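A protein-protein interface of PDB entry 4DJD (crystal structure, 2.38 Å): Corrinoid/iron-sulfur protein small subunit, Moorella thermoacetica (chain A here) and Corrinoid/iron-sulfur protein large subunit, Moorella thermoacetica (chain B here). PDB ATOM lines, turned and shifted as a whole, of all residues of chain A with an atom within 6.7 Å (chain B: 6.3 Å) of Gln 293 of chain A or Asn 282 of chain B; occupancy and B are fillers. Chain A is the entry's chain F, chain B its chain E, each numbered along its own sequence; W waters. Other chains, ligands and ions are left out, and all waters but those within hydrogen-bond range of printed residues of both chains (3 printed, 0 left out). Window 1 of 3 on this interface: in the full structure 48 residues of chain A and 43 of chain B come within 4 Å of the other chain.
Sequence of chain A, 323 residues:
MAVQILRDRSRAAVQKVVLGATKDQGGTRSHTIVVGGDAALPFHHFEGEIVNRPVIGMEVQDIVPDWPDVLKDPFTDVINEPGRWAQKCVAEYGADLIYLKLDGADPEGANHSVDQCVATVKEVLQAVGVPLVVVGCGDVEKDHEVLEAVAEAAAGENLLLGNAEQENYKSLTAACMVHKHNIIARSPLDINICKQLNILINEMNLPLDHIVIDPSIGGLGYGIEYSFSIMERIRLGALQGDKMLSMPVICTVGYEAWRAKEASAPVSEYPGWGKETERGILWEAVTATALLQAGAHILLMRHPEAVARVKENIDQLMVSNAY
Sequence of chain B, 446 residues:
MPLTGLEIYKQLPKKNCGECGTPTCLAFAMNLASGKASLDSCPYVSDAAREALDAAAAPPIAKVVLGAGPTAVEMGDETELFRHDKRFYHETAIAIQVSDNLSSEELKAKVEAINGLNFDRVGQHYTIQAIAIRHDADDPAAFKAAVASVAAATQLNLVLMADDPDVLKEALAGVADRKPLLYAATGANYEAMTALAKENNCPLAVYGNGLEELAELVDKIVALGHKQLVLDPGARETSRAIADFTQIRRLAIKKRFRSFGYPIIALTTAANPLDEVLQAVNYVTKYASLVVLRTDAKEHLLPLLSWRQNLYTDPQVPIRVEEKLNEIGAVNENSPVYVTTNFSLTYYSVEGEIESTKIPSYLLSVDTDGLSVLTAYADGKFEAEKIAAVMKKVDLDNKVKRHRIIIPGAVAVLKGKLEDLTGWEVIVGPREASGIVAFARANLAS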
ATOM      1  N   LEU A  41      -9.955  18.664  35.417  1.00  0.00           N
ATOM      2  CA  LEU A  41     -11.163  19.277  34.873  1.00  0.00           C
ATOM      3  C   LEU A  41     -10.921  19.623  33.403  1.00  0.00           C
ATOM      4  O   LEU A  41      -9.772  19.713  32.974  1.00  0.00           O
ATOM      5  CB  LEU A  41     -11.526  20.532  35.680  1.00  0.00           C
ATOM      6  CG  LEU A  41     -12.096  20.266  37.082  1.00  0.00           C
ATOM      7  CD1 LEU A  41     -12.195  21.550  37.919  1.00  0.00           C
ATOM      8  CD2 LEU A  41     -13.450  19.576  36.981  1.00  0.00           C
ATOM      9  N   PRO A  42     -11.998  19.799  32.620  1.00  0.00           N
ATOM     10  CA  PRO A  42     -11.819  19.990  31.175  1.00  0.00           C
ATOM     11  C   PRO A  42     -10.860  21.125  30.821  1.00  0.00           C
ATOM     12  O   PRO A  42     -11.094  22.270  31.196  1.00  0.00           O
ATOM     13  CB  PRO A  42     -13.235  20.313  30.696  1.00  0.00           C
ATOM     14  CG  PRO A  42     -14.111  19.581  31.649  1.00  0.00           C
ATOM     15  CD  PRO A  42     -13.424  19.690  32.984  1.00  0.00           C
ATOM     16  N   PHE A  43      -9.781  20.779  30.122  1.00  0.00           N
ATOM     17  CA  PHE A  43      -8.787  21.744  29.638  1.00  0.00           C
ATOM     18  C   PHE A  43      -8.051  22.474  30.764  1.00  0.00           C
ATOM     19  O   PHE A  43      -7.501  23.558  30.567  1.00  0.00           O
ATOM     20  CB  PHE A  43      -9.416  22.708  28.625  1.00  0.00           C
ATOM     21  CG  PHE A  43     -10.217  22.004  27.559  1.00  0.00           C
ATOM     22  CD1 PHE A  43      -9.579  21.237  26.591  1.00  0.00           C
ATOM     23  CD2 PHE A  43     -11.602  22.067  27.557  1.00  0.00           C
ATOM     24  CE1 PHE A  43     -10.306  20.565  25.627  1.00  0.00           C
ATOM     25  CE2 PHE A  43     -12.334  21.397  26.602  1.00  0.00           C
ATOM     26  CZ  PHE A  43     -11.685  20.647  25.629  1.00  0.00           C
ATOM     27  N   HIS A  44      -8.029  21.861  31.943  1.00  0.00           N
ATOM     28  CA  HIS A  44      -7.258  22.384  33.066  1.00  0.00           C
ATOM     29  C   HIS A  44      -5.843  21.813  33.051  1.00  0.00           C
ATOM     30  O   HIS A  44      -5.428  21.138  33.995  1.00  0.00           O
ATOM     31  CB  HIS A  44      -7.941  22.062  34.399  1.00  0.00           C
ATOM     32  CG  HIS A  44      -9.151  22.897  34.676  1.00  0.00           C
ATOM     33  ND1 HIS A  44      -9.455  23.372  35.935  1.00  0.00           N
ATOM     34  CD2 HIS A  44     -10.135  23.344  33.860  1.00  0.00           C
ATOM     35  CE1 HIS A  44     -10.574  24.074  35.881  1.00  0.00           C
ATOM     36  NE2 HIS A  44     -11.005  24.071  34.633  1.00  0.00           N
ATOM     37  N   PHE A 228     -25.277  19.329  31.476  1.00  0.00           N
ATOM     38  CA  PHE A 228     -24.016  20.005  31.758  1.00  0.00           C
ATOM     39  C   PHE A 228     -23.573  19.710  33.191  1.00  0.00           C
ATOM     40  O   PHE A 228     -22.426  19.332  33.439  1.00  0.00           O
ATOM     41  CB  PHE A 228     -24.154  21.513  31.526  1.00  0.00           C
ATOM     42  CG  PHE A 228     -22.924  22.304  31.886  1.00  0.00           C
ATOM     43  CD1 PHE A 228     -21.902  22.478  30.964  1.00  0.00           C
ATOM     44  CD2 PHE A 228     -22.796  22.887  33.143  1.00  0.00           C
ATOM     45  CE1 PHE A 228     -20.768  23.206  31.288  1.00  0.00           C
ATOM     46  CE2 PHE A 228     -21.663  23.619  33.476  1.00  0.00           C
ATOM     47  CZ  PHE A 228     -20.648  23.779  32.547  1.00  0.00           C
ATOM     48  N   GLU A 232     -20.435  17.395  34.698  1.00  0.00           N
ATOM     49  CA  GLU A 232     -19.460  17.936  35.636  1.00  0.00           C
ATOM     50  C   GLU A 232     -19.293  16.977  36.815  1.00  0.00           C
ATOM     51  O   GLU A 232     -18.172  16.680  37.237  1.00  0.00           O
ATOM     52  CB  GLU A 232     -19.864  19.333  36.124  1.00  0.00           C
ATOM     53  CG  GLU A 232     -19.684  20.433  35.079  1.00  0.00           C
ATOM     54  CD  GLU A 232     -19.478  21.813  35.691  1.00  0.00           C
ATOM     55  OE1 GLU A 232     -20.368  22.287  36.434  1.00  0.00           O
ATOM     56  OE2 GLU A 232     -18.417  22.423  35.431  1.00  0.00           O
ATOM     57  N   ALA A 288     -22.369  21.899  21.530  1.00  0.00           N
ATOM     58  CA  ALA A 288     -21.137  21.126  21.662  1.00  0.00           C
ATOM     59  C   ALA A 288     -20.111  21.848  22.531  1.00  0.00           C
ATOM     60  O   ALA A 288     -19.463  21.239  23.391  1.00  0.00           O
ATOM     61  CB  ALA A 288     -20.548  20.832  20.288  1.00  0.00           C
ATOM     62  N   THR A 289     -19.977  23.151  22.300  1.00  0.00           N
ATOM     63  CA  THR A 289     -18.986  23.970  22.990  1.00  0.00           C
ATOM     64  C   THR A 289     -19.222  24.014  24.500  1.00  0.00           C
ATOM     65  O   THR A 289     -18.278  23.899  25.283  1.00  0.00           O
ATOM     66  CB  THR A 289     -18.958  25.409  22.424  1.00  0.00           C
ATOM     67  OG1 THR A 289     -18.608  25.368  21.033  1.00  0.00           O
ATOM     68  CG2 THR A 289     -17.948  26.268  23.171  1.00  0.00           C
ATOM     69  N   ALA A 290     -20.478  24.180  24.904  1.00  0.00           N
ATOM     70  CA  ALA A 290     -20.825  24.192  26.323  1.00  0.00           C
ATOM     71  C   ALA A 290     -20.516  22.840  26.957  1.00  0.00           C
ATOM     72  O   ALA A 290     -19.911  22.764  28.021  1.00  0.00           O
ATOM     73  CB  ALA A 290     -22.295  24.547  26.515  1.00  0.00           C
ATOM     74  N   LEU A 291     -20.925  21.772  26.282  1.00  0.00           N
ATOM     75  CA  LEU A 291     -20.710  20.420  26.782  1.00  0.00           C
ATOM     76  C   LEU A 291     -19.233  20.017  26.866  1.00  0.00           C
ATOM     77  O   LEU A 291     -18.861  19.189  27.702  1.00  0.00           O
ATOM     78  CB  LEU A 291     -21.493  19.419  25.932  1.00  0.00           C
ATOM     79  CG  LEU A 291     -23.007  19.497  26.111  1.00  0.00           C
ATOM     80  CD1 LEU A 291     -23.727  18.556  25.145  1.00  0.00           C
ATOM     81  CD2 LEU A 291     -23.372  19.188  27.557  1.00  0.00           C
ATOM     82  N   LEU A 292     -18.393  20.592  26.005  1.00  0.00           N
ATOM     83  CA  LEU A 292     -16.948  20.347  26.078  1.00  0.00           C
ATOM     84  C   LEU A 292     -16.398  20.883  27.392  1.00  0.00           C
ATOM     85  O   LEU A 292     -15.432  20.345  27.933  1.00  0.00           O
ATOM     86  CB  LEU A 292     -16.209  21.002  24.908  1.00  0.00           C
ATOM     87  CG  LEU A 292     -16.232  20.276  23.560  1.00  0.00           C
ATOM     88  CD1 LEU A 292     -15.755  21.203  22.445  1.00  0.00           C
ATOM     89  CD2 LEU A 292     -15.378  19.017  23.609  1.00  0.00           C
ATOM     90  N   GLN A 293     -17.024  21.947  27.898  1.00  0.00           N
ATOM     91  CA  GLN A 293     -16.639  22.538  29.178  1.00  0.00           C
ATOM     92  C   GLN A 293     -17.022  21.643  30.349  1.00  0.00           C
ATOM     93  O   GLN A 293     -16.498  21.799  31.457  1.00  0.00           O
ATOM     94  CB  GLN A 293     -17.268  23.926  29.354  1.00  0.00           C
ATOM     95  CG  GLN A 293     -16.717  24.971  28.394  1.00  0.00           C
ATOM     96  CD  GLN A 293     -15.210  25.117  28.510  1.00  0.00           C
ATOM     97  OE1 GLN A 293     -14.671  25.257  29.609  1.00  0.00           O
ATOM     98  NE2 GLN A 293     -14.520  25.066  27.377  1.00  0.00           N
ATOM     99  N   ALA A 294     -17.933  20.705  30.104  1.00  0.00           N
ATOM    100  CA  ALA A 294     -18.392  19.800  31.157  1.00  0.00           C
ATOM    101  C   ALA A 294     -17.713  18.437  31.071  1.00  0.00           C
ATOM    102  O   ALA A 294     -17.893  17.602  31.947  1.00  0.00           O
ATOM    103  CB  ALA A 294     -19.910  19.649  31.124  1.00  0.00           C
ATOM    104  N   GLY A 295     -16.946  18.207  30.008  1.00  0.00           N
ATOM    105  CA  GLY A 295     -16.130  17.006  29.926  1.00  0.00           C
ATOM    106  C   GLY A 295     -16.472  15.989  28.849  1.00  0.00           C
ATOM    107  O   GLY A 295     -16.285  14.792  29.039  1.00  0.00           O
ATOM    108  N   ALA A 296     -16.962  16.460  27.711  1.00  0.00           N
ATOM    109  CA  ALA A 296     -17.300  15.563  26.612  1.00  0.00           C
ATOM    110  C   ALA A 296     -16.043  15.085  25.886  1.00  0.00           C
ATOM    111  O   ALA A 296     -15.132  15.871  25.631  1.00  0.00           O
ATOM    112  CB  ALA A 296     -18.248  16.251  25.647  1.00  0.00           C
ATOM    113  N   ASN A 313     -12.381  25.512  18.154  1.00  0.00           N
ATOM    114  CA  ASN A 313     -12.547  25.667  19.596  1.00  0.00           C
ATOM    115  C   ASN A 313     -11.649  24.697  20.359  1.00  0.00           C
ATOM    116  O   ASN A 313     -10.894  25.101  21.243  1.00  0.00           O
ATOM    117  CB  ASN A 313     -14.017  25.472  19.985  1.00  0.00           C
ATOM    118  CG  ASN A 313     -14.237  25.543  21.484  1.00  0.00           C
ATOM    119  OD1 ASN A 313     -14.008  26.580  22.104  1.00  0.00           O
ATOM    120  ND2 ASN A 313     -14.694  24.438  22.074  1.00  0.00           N
ATOM    121  N   LEU A 317      -8.405  25.244  22.903  1.00  0.00           N
ATOM    122  CA  LEU A 317      -8.509  24.755  24.270  1.00  0.00           C
ATOM    123  C   LEU A 317      -7.427  23.735  24.609  1.00  0.00           C
ATOM    124  O   LEU A 317      -7.067  23.572  25.774  1.00  0.00           O
ATOM    125  CB  LEU A 317      -9.895  24.151  24.512  1.00  0.00           C
ATOM    126  CG  LEU A 317     -11.055  25.144  24.588  1.00  0.00           C
ATOM    127  CD1 LEU A 317     -12.387  24.419  24.589  1.00  0.00           C
ATOM    128  CD2 LEU A 317     -10.915  26.003  25.827  1.00  0.00           C
ATOM    129  N   THR B 238      -8.104  31.752  24.464  1.00  0.00           N
ATOM    130  CA  THR B 238      -9.146  31.018  25.177  1.00  0.00           C
ATOM    131  C   THR B 238      -8.626  30.171  26.334  1.00  0.00           C
ATOM    132  O   THR B 238      -9.159  30.231  27.441  1.00  0.00           O
ATOM    133  CB  THR B 238      -9.948  30.126  24.216  1.00  0.00           C
ATOM    134  OG1 THR B 238     -10.455  30.925  23.137  1.00  0.00           O
ATOM    135  CG2 THR B 238     -11.116  29.468  24.948  1.00  0.00           C
ATOM    136  N   ILE B 242      -9.491  30.893  30.393  1.00  0.00           N
ATOM    137  CA  ILE B 242     -10.203  29.939  31.230  1.00  0.00           C
ATOM    138  C   ILE B 242      -9.414  29.576  32.495  1.00  0.00           C
ATOM    139  O   ILE B 242      -9.987  29.442  33.574  1.00  0.00           O
ATOM    140  CB  ILE B 242     -10.580  28.686  30.409  1.00  0.00           C
ATOM    141  CG1 ILE B 242     -11.696  29.049  29.423  1.00  0.00           C
ATOM    142  CG2 ILE B 242     -10.992  27.536  31.313  1.00  0.00           C
ATOM    143  CD1 ILE B 242     -12.234  27.882  28.634  1.00  0.00           C
ATOM    144  N   PHE B 245      -9.316  32.966  34.685  1.00  0.00           N
ATOM    145  CA  PHE B 245     -10.607  33.250  35.308  1.00  0.00           C
ATOM    146  C   PHE B 245     -10.879  32.246  36.425  1.00  0.00           C
ATOM    147  O   PHE B 245     -11.420  32.602  37.474  1.00  0.00           O
ATOM    148  CB  PHE B 245     -11.752  33.217  34.285  1.00  0.00           C
ATOM    149  CG  PHE B 245     -11.604  34.210  33.158  1.00  0.00           C
ATOM    150  CD1 PHE B 245     -10.718  35.275  33.253  1.00  0.00           C
ATOM    151  CD2 PHE B 245     -12.357  34.075  32.001  1.00  0.00           C
ATOM    152  CE1 PHE B 245     -10.585  36.186  32.217  1.00  0.00           C
ATOM    153  CE2 PHE B 245     -12.229  34.985  30.958  1.00  0.00           C
ATOM    154  CZ  PHE B 245     -11.343  36.040  31.066  1.00  0.00           C
ATOM    155  N   VAL B 277     -18.317  33.815  18.972  1.00  0.00           N
ATOM    156  CA  VAL B 277     -19.451  33.353  19.761  1.00  0.00           C
ATOM    157  C   VAL B 277     -19.049  32.183  20.656  1.00  0.00           C
ATOM    158  O   VAL B 277     -19.348  32.187  21.851  1.00  0.00           O
ATOM    159  CB  VAL B 277     -20.668  32.974  18.873  1.00  0.00           C
ATOM    160  CG1 VAL B 277     -21.732  32.238  19.691  1.00  0.00           C
ATOM    161  CG2 VAL B 277     -21.262  34.217  18.238  1.00  0.00           C
ATOM    162  N   LEU B 278     -18.350  31.202  20.089  1.00  0.00           N
ATOM    163  CA  LEU B 278     -17.927  30.029  20.858  1.00  0.00           C
ATOM    164  C   LEU B 278     -16.971  30.417  21.982  1.00  0.00           C
ATOM    165  O   LEU B 278     -17.028  29.873  23.089  1.00  0.00           O
ATOM    166  CB  LEU B 278     -17.272  28.982  19.953  1.00  0.00           C
ATOM    167  CG  LEU B 278     -18.144  28.411  18.836  1.00  0.00           C
ATOM    168  CD1 LEU B 278     -17.512  27.138  18.278  1.00  0.00           C
ATOM    169  CD2 LEU B 278     -19.560  28.162  19.339  1.00  0.00           C
ATOM    170  N   GLN B 279     -16.093  31.363  21.681  1.00  0.00           N
ATOM    171  CA  GLN B 279     -15.195  31.932  22.677  1.00  0.00           C
ATOM    172  C   GLN B 279     -16.005  32.580  23.800  1.00  0.00           C
ATOM    173  O   GLN B 279     -15.705  32.412  24.982  1.00  0.00           O
ATOM    174  CB  GLN B 279     -14.284  32.961  22.014  1.00  0.00           C
ATOM    175  CG  GLN B 279     -13.040  33.297  22.797  1.00  0.00           C
ATOM    176  CD  GLN B 279     -12.057  34.115  21.983  1.00  0.00           C
ATOM    177  OE1 GLN B 279     -12.447  35.018  21.246  1.00  0.00           O
ATOM    178  NE2 GLN B 279     -10.777  33.790  22.103  1.00  0.00           N
ATOM    179  N   ALA B 280     -17.050  33.308  23.423  1.00  0.00           N
ATOM    180  CA  ALA B 280     -17.934  33.930  24.400  1.00  0.00           C
ATOM    181  C   ALA B 280     -18.651  32.921  25.302  1.00  0.00           C
ATOM    182  O   ALA B 280     -18.799  33.182  26.491  1.00  0.00           O
ATOM    183  CB  ALA B 280     -18.934  34.851  23.719  1.00  0.00           C
ATOM    184  N   VAL B 281     -19.083  31.772  24.769  1.00  0.00           N
ATOM    185  CA  VAL B 281     -19.749  30.787  25.637  1.00  0.00           C
ATOM    186  C   VAL B 281     -18.785  30.146  26.635  1.00  0.00           C
ATOM    187  O   VAL B 281     -19.173  29.820  27.757  1.00  0.00           O
ATOM    188  CB  VAL B 281     -20.596  29.704  24.878  1.00  0.00           C
ATOM    189  CG1 VAL B 281     -20.630  29.959  23.406  1.00  0.00           C
ATOM    190  CG2 VAL B 281     -20.116  28.287  25.181  1.00  0.00           C
ATOM    191  N   ASN B 282     -17.530  29.981  26.227  1.00  0.00           N
ATOM    192  CA  ASN B 282     -16.490  29.540  27.144  1.00  0.00           C
ATOM    193  C   ASN B 282     -16.349  30.521  28.295  1.00  0.00           C
ATOM    194  O   ASN B 282     -16.263  30.123  29.456  1.00  0.00           O
ATOM    195  CB  ASN B 282     -15.155  29.391  26.412  1.00  0.00           C
ATOM    196  CG  ASN B 282     -15.113  28.156  25.533  1.00  0.00           C
ATOM    197  OD1 ASN B 282     -15.566  27.085  25.930  1.00  0.00           O
ATOM    198  ND2 ASN B 282     -14.581  28.303  24.329  1.00  0.00           N
ATOM    199  N   TYR B 283     -16.357  31.808  27.965  1.00  0.00           N
ATOM    200  CA  TYR B 283     -16.148  32.848  28.962  1.00  0.00           C
ATOM    201  C   TYR B 283     -17.319  32.981  29.932  1.00  0.00           C
ATOM    202  O   TYR B 283     -17.104  33.144  31.132  1.00  0.00           O
ATOM    203  CB  TYR B 283     -15.815  34.190  28.301  1.00  0.00           C
ATOM    204  CG  TYR B 283     -14.494  34.181  27.557  1.00  0.00           C
ATOM    205  CD1 TYR B 283     -13.604  33.121  27.698  1.00  0.00           C
ATOM    206  CD2 TYR B 283     -14.136  35.227  26.717  1.00  0.00           C
ATOM    207  CE1 TYR B 283     -12.403  33.098  27.021  1.00  0.00           C
ATOM    208  CE2 TYR B 283     -12.930  35.217  26.038  1.00  0.00           C
ATOM    209  CZ  TYR B 283     -12.066  34.150  26.193  1.00  0.00           C
ATOM    210  OH  TYR B 283     -10.862  34.127  25.521  1.00  0.00           O
ATOM    211  N   VAL B 284     -18.555  32.894  29.441  1.00  0.00           N
ATOM    212  CA  VAL B 284     -19.683  32.950  30.368  1.00  0.00           C
ATOM    213  C   VAL B 284     -19.712  31.699  31.243  1.00  0.00           C
ATOM    214  O   VAL B 284     -20.143  31.756  32.391  1.00  0.00           O
ATOM    215  CB  VAL B 284     -21.077  33.200  29.692  1.00  0.00           C
ATOM    216  CG1 VAL B 284     -20.948  34.079  28.456  1.00  0.00           C
ATOM    217  CG2 VAL B 284     -21.784  31.902  29.383  1.00  0.00           C
ATOM    218  N   THR B 285     -19.234  30.578  30.704  1.00  0.00           N
ATOM    219  CA  THR B 285     -19.192  29.328  31.461  1.00  0.00           C
ATOM    220  C   THR B 285     -18.163  29.437  32.574  1.00  0.00           C
ATOM    221  O   THR B 285     -18.410  29.011  33.707  1.00  0.00           O
ATOM    222  CB  THR B 285     -18.808  28.121  30.579  1.00  0.00           C
ATOM    223  OG1 THR B 285     -19.706  28.021  29.469  1.00  0.00           O
ATOM    224  CG2 THR B 285     -18.860  26.822  31.396  1.00  0.00           C
ATOM    225  N   LYS B 286     -17.014  30.021  32.241  1.00  0.00           N
ATOM    226  CA  LYS B 286     -15.893  30.116  33.167  1.00  0.00           C
ATOM    227  C   LYS B 286     -15.757  31.488  33.826  1.00  0.00           C
ATOM    228  O   LYS B 286     -14.699  32.122  33.749  1.00  0.00           O
ATOM    229  CB  LYS B 286     -14.579  29.741  32.473  1.00  0.00           C
ATOM    230  CG  LYS B 286     -14.589  28.373  31.801  1.00  0.00           C
ATOM    231  CD  LYS B 286     -15.126  27.284  32.728  1.00  0.00           C
ATOM    232  CE  LYS B 286     -14.140  26.930  33.827  1.00  0.00           C
ATOM    233  NZ  LYS B 286     -14.712  25.924  34.767  1.00  0.00           N
ATOM    234  N   TYR B 287     -16.840  31.943  34.454  1.00  0.00           N
ATOM    235  CA  TYR B 287     -16.777  32.962  35.511  1.00  0.00           C
ATOM    236  C   TYR B 287     -16.653  34.427  35.088  1.00  0.00           C
ATOM    237  O   TYR B 287     -16.559  35.299  35.948  1.00  0.00           O
ATOM    238  CB  TYR B 287     -15.669  32.614  36.515  1.00  0.00           C
ATOM    239  CG  TYR B 287     -15.667  31.156  36.913  1.00  0.00           C
ATOM    240  CD1 TYR B 287     -16.831  30.539  37.352  1.00  0.00           C
ATOM    241  CD2 TYR B 287     -14.510  30.385  36.816  1.00  0.00           C
ATOM    242  CE1 TYR B 287     -16.843  29.202  37.711  1.00  0.00           C
ATOM    243  CE2 TYR B 287     -14.513  29.045  37.170  1.00  0.00           C
ATOM    244  CZ  TYR B 287     -15.683  28.460  37.618  1.00  0.00           C
ATOM    245  OH  TYR B 287     -15.706  27.131  37.975  1.00  0.00           O
ATOM    246  N   TRP B 307     -27.619  30.219  26.114  1.00  0.00           N
ATOM    247  CA  TRP B 307     -26.728  29.468  26.987  1.00  0.00           C
ATOM    248  C   TRP B 307     -26.567  30.152  28.339  1.00  0.00           C
ATOM    249  O   TRP B 307     -26.589  29.494  29.385  1.00  0.00           O
ATOM    250  CB  TRP B 307     -25.357  29.260  26.328  1.00  0.00           C
ATOM    251  CG  TRP B 307     -24.326  28.742  27.286  1.00  0.00           C
ATOM    252  CD1 TRP B 307     -23.150  29.343  27.624  1.00  0.00           C
ATOM    253  CD2 TRP B 307     -24.390  27.530  28.054  1.00  0.00           C
ATOM    254  NE1 TRP B 307     -22.471  28.578  28.542  1.00  0.00           N
ATOM    255  CE2 TRP B 307     -23.210  27.456  28.820  1.00  0.00           C
ATOM    256  CE3 TRP B 307     -25.329  26.494  28.156  1.00  0.00           C
ATOM    257  CZ2 TRP B 307     -22.943  26.396  29.686  1.00  0.00           C
ATOM    258  CZ3 TRP B 307     -25.062  25.437  29.020  1.00  0.00           C
ATOM    259  CH2 TRP B 307     -23.879  25.398  29.774  1.00  0.00           C
HETATM  260  O   HOH W   1     -12.925  29.261  21.603  1.00  0.00           O
HETATM  261  O   HOH W   2     -17.770  24.978  36.321  1.00  0.00           O
HETATM  262  O   HOH W   3     -15.648  24.552  24.889  1.00  0.00           O
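ND2 of Asn 282 of chain B sits at hydrogen-bond distance from OD1 of Asn 313 of chain A (2.9 Å). The side-chain amide nitrogen of Gln 293 of chain A is in hydrogen-bond range of the side-chain amide oxygen of Asn 282 of chain B.
The backbone carbonyl oxygen (O) of Val 281 of chain B is in hydrogen-bond range of the side-chain hydroxyl (OG1) of Thr 285 of chain B (2.5 Å). OG1 of Thr 285 of chain B lies within hydrogen-bond range of NE1 of Trp 307 of chain B (3.0 Å). The side-chain hydroxyl (OG1) of Thr 238 of chain B sits at hydrogen-bond distance from the side-chain amide nitrogen (NE2) of Gln 279 of chain B, 3.1 Å away. The side-chain amide nitrogen (ND2) of Asn 282 of chain B lies within hydrogen-bond range of the backbone carbonyl oxygen (O) of Leu 278 of chain B, 3.2 Å away.
Of chain B, only Ile 242 (3.7 Å), Asn 282 (2.7 Å), Thr 285 (3.9 Å) and Lys 286 (3.7 Å) come within 4 Å of Gln 293 of chain A. Of the printed residues of chain A, Thr 285 of chain B touches Phe 228 and Gln 293. Printed residues of chain A within 4 Å of Lys 286 of chain B: Gln 293.
Among the printed residues, pairs that only touch across the chains: Phe 228 of chain A with Thr 285 of chain B, Phe 228 of chain A with Trp 307 of chain B, Thr 289 of chain A with Leu 278 of chain B, Thr 289 of chain A with Val 281 of chain B, Thr 289 of chain A with Asn 282 of chain B, Ala 290 of chain A with Trp 307 of chain B, Gln 293 of chain A with Ile 242 of chain B, Gln 293 of chain A with Thr 285 of chain B, Gln 293 of chain A with Lys 286 of chain B, Leu 317 of chain A with Thr 238 of chain B and Leu 317 of chain A with Ile 242 of chain B.
Water W3 lies within hydrogen-bond range of the backbone carbonyl oxygen of Thr 289 of chain A (2.7 Å), the side-chain amide oxygen of Asn 282 of chain B (2.7 Å), the side-chain amide nitrogen of Gln 293 of chain A (2.8 Å) and the side-chain amide nitrogen of Asn 313 of chain A (3.0 Å). Water W2 bridges OE2 of Glu 232 of chain A and OH of Tyr 287 of chain B. Water W1 lies within hydrogen-bond range of OD1 of Asn 313 of chain A, ND2 of Asn 282 of chain B and OG1 of Thr 238 of chain B.
Hydrophobic or aromatic side chains of chain A that line the printed part of chain B: Phe 228, Ala 290 and Leu 317. Of the 15 printed residues of chain B, 8 touch a printed residue of chain A. Hydrophobic or aromatic side chains of chain B within 4 Å of the printed part of chain A: Ile 242, Leu 278, Val 281 and Trp 307.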
